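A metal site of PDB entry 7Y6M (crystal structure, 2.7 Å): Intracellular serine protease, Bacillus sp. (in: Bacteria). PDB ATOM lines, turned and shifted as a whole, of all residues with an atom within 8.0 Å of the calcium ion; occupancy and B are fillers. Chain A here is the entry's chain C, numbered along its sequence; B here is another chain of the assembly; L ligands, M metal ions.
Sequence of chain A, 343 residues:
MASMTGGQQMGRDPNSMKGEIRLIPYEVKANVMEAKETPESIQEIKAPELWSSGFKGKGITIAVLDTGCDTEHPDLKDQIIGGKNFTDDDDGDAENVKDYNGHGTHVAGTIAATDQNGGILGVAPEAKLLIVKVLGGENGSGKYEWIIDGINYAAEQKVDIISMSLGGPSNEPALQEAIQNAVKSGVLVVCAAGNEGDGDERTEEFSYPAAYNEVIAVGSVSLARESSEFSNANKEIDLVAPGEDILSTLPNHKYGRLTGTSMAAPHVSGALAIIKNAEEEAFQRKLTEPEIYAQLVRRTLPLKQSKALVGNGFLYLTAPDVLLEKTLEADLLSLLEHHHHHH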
ATOM      1  N   VAL A 189       6.212  27.386  -2.827  1.00  0.00           N
ATOM      2  CA  VAL A 189       5.970  26.640  -1.592  1.00  0.00           C
ATOM      3  C   VAL A 189       7.111  26.913  -0.609  1.00  0.00           C
ATOM      4  O   VAL A 189       8.227  26.412  -0.783  1.00  0.00           O
ATOM      5  CB  VAL A 189       5.832  25.153  -1.901  1.00  0.00           C
ATOM      6  CG1 VAL A 189       5.651  24.365  -0.626  1.00  0.00           C
ATOM      7  CG2 VAL A 189       4.654  24.959  -2.847  1.00  0.00           C
ATOM      8  N   PRO A 209       8.135  19.394   5.333  1.00  0.00           N
ATOM      9  CA  PRO A 209       8.507  19.357   3.914  1.00  0.00           C
ATOM     10  C   PRO A 209       9.738  20.153   3.481  1.00  0.00           C
ATOM     11  O   PRO A 209      10.157  19.961   2.341  1.00  0.00           O
ATOM     12  CB  PRO A 209       7.268  19.913   3.234  1.00  0.00           C
ATOM     13  CG  PRO A 209       6.683  20.835   4.213  1.00  0.00           C
ATOM     14  CD  PRO A 209       6.941  20.231   5.557  1.00  0.00           C
ATOM     15  N   ALA A 210      10.306  20.988   4.359  1.00  0.00           N
ATOM     16  CA  ALA A 210      11.475  21.810   4.007  1.00  0.00           C
ATOM     17  C   ALA A 210      12.555  21.058   3.224  1.00  0.00           C
ATOM     18  O   ALA A 210      13.090  21.552   2.228  1.00  0.00           O
ATOM     19  CB  ALA A 210      12.094  22.380   5.276  1.00  0.00           C
ATOM     20  N   ALA A 211      12.897  19.847   3.663  1.00  0.00           N
ATOM     21  CA  ALA A 211      13.988  19.103   3.062  1.00  0.00           C
ATOM     22  C   ALA A 211      13.768  18.739   1.581  1.00  0.00           C
ATOM     23  O   ALA A 211      14.717  18.271   0.940  1.00  0.00           O
ATOM     24  CB  ALA A 211      14.229  17.831   3.900  1.00  0.00           C
ATOM     25  N   TYR A 212      12.562  18.924   1.034  1.00  0.00           N
ATOM     26  CA  TYR A 212      12.352  18.587  -0.370  1.00  0.00           C
ATOM     27  C   TYR A 212      12.911  19.685  -1.261  1.00  0.00           C
ATOM     28  O   TYR A 212      12.699  20.869  -1.011  1.00  0.00           O
ATOM     29  CB  TYR A 212      10.864  18.421  -0.673  1.00  0.00           C
ATOM     30  CG  TYR A 212      10.189  17.252  -0.010  1.00  0.00           C
ATOM     31  CD1 TYR A 212      10.667  15.965  -0.185  1.00  0.00           C
ATOM     32  CD2 TYR A 212       9.060  17.442   0.780  1.00  0.00           C
ATOM     33  CE1 TYR A 212      10.058  14.910   0.427  1.00  0.00           C
ATOM     34  CE2 TYR A 212       8.445  16.395   1.383  1.00  0.00           C
ATOM     35  CZ  TYR A 212       8.930  15.127   1.198  1.00  0.00           C
ATOM     36  OH  TYR A 212       8.293  14.080   1.804  1.00  0.00           O
ATOM     37  N   ASN A 213      13.622  19.269  -2.320  1.00  0.00           N
ATOM     38  CA  ASN A 213      14.341  20.272  -3.095  1.00  0.00           C
ATOM     39  C   ASN A 213      13.402  21.374  -3.575  1.00  0.00           C
ATOM     40  O   ASN A 213      13.800  22.537  -3.613  1.00  0.00           O
ATOM     41  CB  ASN A 213      15.069  19.647  -4.276  1.00  0.00           C
ATOM     42  CG  ASN A 213      15.842  20.683  -5.087  1.00  0.00           C
ATOM     43  OD1 ASN A 213      15.293  21.316  -5.982  1.00  0.00           O
ATOM     44  ND2 ASN A 213      17.103  20.883  -4.757  1.00  0.00           N
ATOM     45  N   GLU A 214      12.144  21.055  -3.894  1.00  0.00           N
ATOM     46  CA  GLU A 214      11.278  22.078  -4.463  1.00  0.00           C
ATOM     47  C   GLU A 214      10.960  23.192  -3.464  1.00  0.00           C
ATOM     48  O   GLU A 214      10.745  24.340  -3.871  1.00  0.00           O
ATOM     49  CB  GLU A 214       9.963  21.476  -4.958  1.00  0.00           C
ATOM     50  CG  GLU A 214      10.103  20.245  -5.769  1.00  0.00           C
ATOM     51  CD  GLU A 214       9.781  19.021  -4.956  1.00  0.00           C
ATOM     52  OE1 GLU A 214       8.613  18.558  -4.992  1.00  0.00           O
ATOM     53  OE2 GLU A 214      10.725  18.532  -4.282  1.00  0.00           O
ATOM     54  N   VAL A 215      10.879  22.868  -2.176  1.00  0.00           N
ATOM     55  CA  VAL A 215      10.449  23.852  -1.202  1.00  0.00           C
ATOM     56  C   VAL A 215      11.456  24.983  -1.138  1.00  0.00           C
ATOM     57  O   VAL A 215      12.654  24.786  -1.378  1.00  0.00           O
ATOM     58  CB  VAL A 215      10.270  23.187   0.172  1.00  0.00           C
ATOM     59  CG1 VAL A 215       9.717  24.154   1.168  1.00  0.00           C
ATOM     60  CG2 VAL A 215       9.361  21.971   0.038  1.00  0.00           C
ATOM     61  N   ILE A 216      10.990  26.198  -0.866  1.00  0.00           N
ATOM     62  CA  ILE A 216      11.894  27.280  -0.494  1.00  0.00           C
ATOM     63  C   ILE A 216      12.081  27.150   1.018  1.00  0.00           C
ATOM     64  O   ILE A 216      11.335  27.714   1.815  1.00  0.00           O
ATOM     65  CB  ILE A 216      11.386  28.656  -0.918  1.00  0.00           C
ATOM     66  CG1 ILE A 216      10.863  28.599  -2.374  1.00  0.00           C
ATOM     67  CG2 ILE A 216      12.491  29.686  -0.805  1.00  0.00           C
ATOM     68  CD1 ILE A 216      10.592  29.953  -3.014  1.00  0.00           C
ATOM     69  N   ALA A 217      13.083  26.376   1.403  1.00  0.00           N
ATOM     70  CA  ALA A 217      13.389  26.133   2.810  1.00  0.00           C
ATOM     71  C   ALA A 217      14.130  27.329   3.398  1.00  0.00           C
ATOM     72  O   ALA A 217      15.169  27.745   2.877  1.00  0.00           O
ATOM     73  CB  ALA A 217      14.236  24.878   2.958  1.00  0.00           C
ATOM     74  N   VAL A 218      13.601  27.841   4.514  1.00  0.00           N
ATOM     75  CA  VAL A 218      14.082  29.077   5.114  1.00  0.00           C
ATOM     76  C   VAL A 218      14.653  28.779   6.483  1.00  0.00           C
ATOM     77  O   VAL A 218      13.927  28.366   7.390  1.00  0.00           O
ATOM     78  CB  VAL A 218      12.974  30.144   5.208  1.00  0.00           C
ATOM     79  CG1 VAL A 218      13.562  31.457   5.684  1.00  0.00           C
ATOM     80  CG2 VAL A 218      12.266  30.309   3.847  1.00  0.00           C
ATOM     81  N   LYS A 235      21.544  20.203   2.927  1.00  0.00           N
ATOM     82  CA  LYS A 235      21.927  20.722   1.621  1.00  0.00           C
ATOM     83  C   LYS A 235      20.748  21.283   0.868  1.00  0.00           C
ATOM     84  O   LYS A 235      20.839  21.470  -0.346  1.00  0.00           O
ATOM     85  CB  LYS A 235      22.619  19.630   0.801  1.00  0.00           C
ATOM     86  CG  LYS A 235      23.899  19.115   1.427  1.00  0.00           C
ATOM     87  CD  LYS A 235      24.816  18.471   0.387  1.00  0.00           C
ATOM     88  CE  LYS A 235      26.159  18.055   0.994  1.00  0.00           C
ATOM     89  NZ  LYS A 235      26.156  16.701   1.654  1.00  0.00           N
ATOM     90  N   GLU A 236      19.638  21.524   1.556  1.00  0.00           N
ATOM     91  CA  GLU A 236      18.410  21.988   0.926  1.00  0.00           C
ATOM     92  C   GLU A 236      17.926  23.309   1.509  1.00  0.00           C
ATOM     93  O   GLU A 236      16.777  23.722   1.266  1.00  0.00           O
ATOM     94  CB  GLU A 236      17.335  20.912   1.031  1.00  0.00           C
ATOM     95  CG  GLU A 236      17.695  19.622   0.358  1.00  0.00           C
ATOM     96  CD  GLU A 236      17.935  19.808  -1.112  1.00  0.00           C
ATOM     97  OE1 GLU A 236      17.306  20.746  -1.666  1.00  0.00           O
ATOM     98  OE2 GLU A 236      18.748  19.040  -1.711  1.00  0.00           O
ATOM     99  N   ILE A 237      18.765  23.992   2.275  1.00  0.00           N
ATOM    100  CA  ILE A 237      18.509  25.361   2.684  1.00  0.00           C
ATOM    101  C   ILE A 237      18.621  26.262   1.464  1.00  0.00           C
ATOM    102  O   ILE A 237      19.603  26.202   0.720  1.00  0.00           O
ATOM    103  CB  ILE A 237      19.491  25.772   3.798  1.00  0.00           C
ATOM    104  CG1 ILE A 237      19.599  24.661   4.831  1.00  0.00           C
ATOM    105  CG2 ILE A 237      19.089  27.109   4.454  1.00  0.00           C
ATOM    106  CD1 ILE A 237      18.277  24.309   5.531  1.00  0.00           C
ATOM    107  N   ASP A 238      17.607  27.113   1.251  1.00  0.00           N
ATOM    108  CA  ASP A 238      17.659  28.067   0.142  1.00  0.00           C
ATOM    109  C   ASP A 238      18.192  29.424   0.586  1.00  0.00           C
ATOM    110  O   ASP A 238      19.057  30.021  -0.084  1.00  0.00           O
ATOM    111  CB  ASP A 238      16.270  28.247  -0.467  1.00  0.00           C
ATOM    112  CG  ASP A 238      15.688  26.944  -0.988  1.00  0.00           C
ATOM    113  OD1 ASP A 238      15.922  26.642  -2.153  1.00  0.00           O
ATOM    114  OD2 ASP A 238      14.973  26.244  -0.231  1.00  0.00           O
ATOM    115  N   LEU A 239      17.670  29.954   1.692  1.00  0.00           N
ATOM    116  CA  LEU A 239      18.086  31.247   2.228  1.00  0.00           C
ATOM    117  C   LEU A 239      17.666  31.300   3.681  1.00  0.00           C
ATOM    118  O   LEU A 239      16.994  30.404   4.178  1.00  0.00           O
ATOM    119  CB  LEU A 239      17.495  32.410   1.428  1.00  0.00           C
ATOM    120  CG  LEU A 239      16.010  32.731   1.695  1.00  0.00           C
ATOM    121  CD1 LEU A 239      15.574  33.976   0.937  1.00  0.00           C
ATOM    122  CD2 LEU A 239      15.091  31.564   1.353  1.00  0.00           C
ATOM    123  N   TYR A 293      11.716  32.468  -8.114  1.00  0.00           N
ATOM    124  CA  TYR A 293      12.736  31.889  -7.235  1.00  0.00           C
ATOM    125  C   TYR A 293      14.107  32.491  -7.527  1.00  0.00           C
ATOM    126  O   TYR A 293      14.800  32.968  -6.615  1.00  0.00           O
ATOM    127  CB  TYR A 293      12.778  30.358  -7.378  1.00  0.00           C
ATOM    128  CG  TYR A 293      13.922  29.708  -6.605  1.00  0.00           C
ATOM    129  CD1 TYR A 293      13.947  29.716  -5.203  1.00  0.00           C
ATOM    130  CD2 TYR A 293      14.993  29.106  -7.260  1.00  0.00           C
ATOM    131  CE1 TYR A 293      14.988  29.136  -4.481  1.00  0.00           C
ATOM    132  CE2 TYR A 293      16.036  28.523  -6.552  1.00  0.00           C
ATOM    133  CZ  TYR A 293      16.027  28.547  -5.166  1.00  0.00           C
ATOM    134  OH  TYR A 293      17.054  27.976  -4.448  1.00  0.00           O
ATOM    135  N   ASN A 312      21.595  30.472   0.384  1.00  0.00           N
ATOM    136  CA  ASN A 312      22.182  31.486  -0.471  1.00  0.00           C
ATOM    137  C   ASN A 312      22.616  32.701   0.324  1.00  0.00           C
ATOM    138  O   ASN A 312      23.535  33.423  -0.095  1.00  0.00           O
ATOM    139  CB  ASN A 312      21.179  31.904  -1.533  1.00  0.00           C
ATOM    140  CG  ASN A 312      21.150  30.962  -2.713  1.00  0.00           C
ATOM    141  OD1 ASN A 312      22.015  31.026  -3.587  1.00  0.00           O
ATOM    142  ND2 ASN A 312      20.151  30.099  -2.765  1.00  0.00           N
ATOM    143  N   ARG B 285      26.556  19.488  -3.562  1.00  0.00           N
ATOM    144  CA  ARG B 285      25.645  18.547  -4.191  1.00  0.00           C
ATOM    145  C   ARG B 285      25.525  18.945  -5.647  1.00  0.00           C
ATOM    146  O   ARG B 285      26.188  19.882  -6.096  1.00  0.00           O
ATOM    147  CB  ARG B 285      24.275  18.509  -3.498  1.00  0.00           C
ATOM    148  CG  ARG B 285      23.510  19.851  -3.331  1.00  0.00           C
ATOM    149  CD  ARG B 285      22.010  19.564  -3.137  1.00  0.00           C
ATOM    150  NE  ARG B 285      21.183  20.703  -2.763  1.00  0.00           N
ATOM    151  CZ  ARG B 285      20.503  21.464  -3.624  1.00  0.00           C
ATOM    152  NH1 ARG B 285      20.584  21.230  -4.942  1.00  0.00           N
ATOM    153  NH2 ARG B 285      19.758  22.486  -3.184  1.00  0.00           N
ATOM    154  N   THR B 288      19.792  21.486  -9.528  1.00  0.00           N
ATOM    155  CA  THR B 288      18.773  21.269 -10.541  1.00  0.00           C
ATOM    156  C   THR B 288      18.749  22.443 -11.524  1.00  0.00           C
ATOM    157  O   THR B 288      19.361  23.499 -11.305  1.00  0.00           O
ATOM    158  CB  THR B 288      17.383  21.085  -9.915  1.00  0.00           C
ATOM    159  OG1 THR B 288      16.787  22.365  -9.711  1.00  0.00           O
ATOM    160  CG2 THR B 288      17.492  20.429  -8.611  1.00  0.00           C
ATOM    161  N   GLU B 291      17.546  25.662 -10.023  1.00  0.00           N
ATOM    162  CA  GLU B 291      18.561  26.247  -9.152  1.00  0.00           C
ATOM    163  C   GLU B 291      19.693  26.871  -9.958  1.00  0.00           C
ATOM    164  O   GLU B 291      20.165  27.971  -9.615  1.00  0.00           O
ATOM    165  CB  GLU B 291      19.144  25.194  -8.216  1.00  0.00           C
ATOM    166  CG  GLU B 291      18.216  24.598  -7.241  1.00  0.00           C
ATOM    167  CD  GLU B 291      18.896  23.469  -6.531  1.00  0.00           C
ATOM    168  OE1 GLU B 291      18.990  23.518  -5.280  1.00  0.00           O
ATOM    169  OE2 GLU B 291      19.385  22.546  -7.217  1.00  0.00           O
HETATM  170  C1  LIG L   1      13.474  26.070  -6.434  1.00  0.00           C
HETATM  171  O1  LIG L   1      12.358  25.661  -7.238  1.00  0.00           O
HETATM  172  C2  LIG L   1      13.085  25.978  -4.844  1.00  0.00           C
HETATM  173  O2  LIG L   1      14.243  25.581  -4.034  1.00  0.00           O
HETATM  174  C3  LIG L   1      15.229  24.801  -4.803  1.00  0.00           C
HETATM  175  C4  LIG L   1      16.639  24.768  -4.127  1.00  0.00           C
HETATM  176  O3  LIG L   1      16.747  23.773  -3.081  1.00  0.00           O
HETATM  177 CA    CA M   1      14.874  24.323  -2.180  1.00  0.00          CA
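The side-chain carboxylate (OE1) of Glu 236 is in hydrogen-bond range of the side-chain amide nitrogen (ND2) of Asn 213, at 3.1 Å. The side-chain amide nitrogen (ND2) of Asn 213 sits at hydrogen-bond distance from the side-chain carboxylate (OE1) of Glu 291 of chain B. The side-chain amide nitrogen (ND2) of Asn 213 lies close to the guanidinium group (NH2) of Arg 285 of chain B (3.5 Å). N of Asp 238 is in hydrogen-bond range of O of Ala 217 (3.0 Å). The side-chain carboxylate (OD1) of Asp 238 lies close to the side-chain hydroxyl (OH) of Tyr 293, at 2.9 Å. The backbone NH (N) of Asn 312 is in hydrogen-bond range of the backbone carbonyl oxygen (O) of Asp 238 (2.6 Å). The guanidinium group (NE) of Arg 285 of chain B is in salt-bridge range of the side-chain carboxylate (OE2) of Glu 236 (3.1 Å).
Glu 236 touches the calcium ion. Within 4 Å of the calcium ion: Asn 213, Val 215, Glu 236 and Asp 238.
The calcium ion is bound by an oxygen (O3) of the ligand (2.1 Å), an oxygen (O2) of the ligand (2.3 Å), the backbone carbonyl oxygen (O) of Val 215 (2.4 Å), the backbone carbonyl oxygen (O) of Asn 213 (2.5 Å), the side-chain carboxylate (OD1) of Asp 238 (2.5 Å) and the side-chain carboxylate (OD2) of Asp 238 (2.7 Å).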
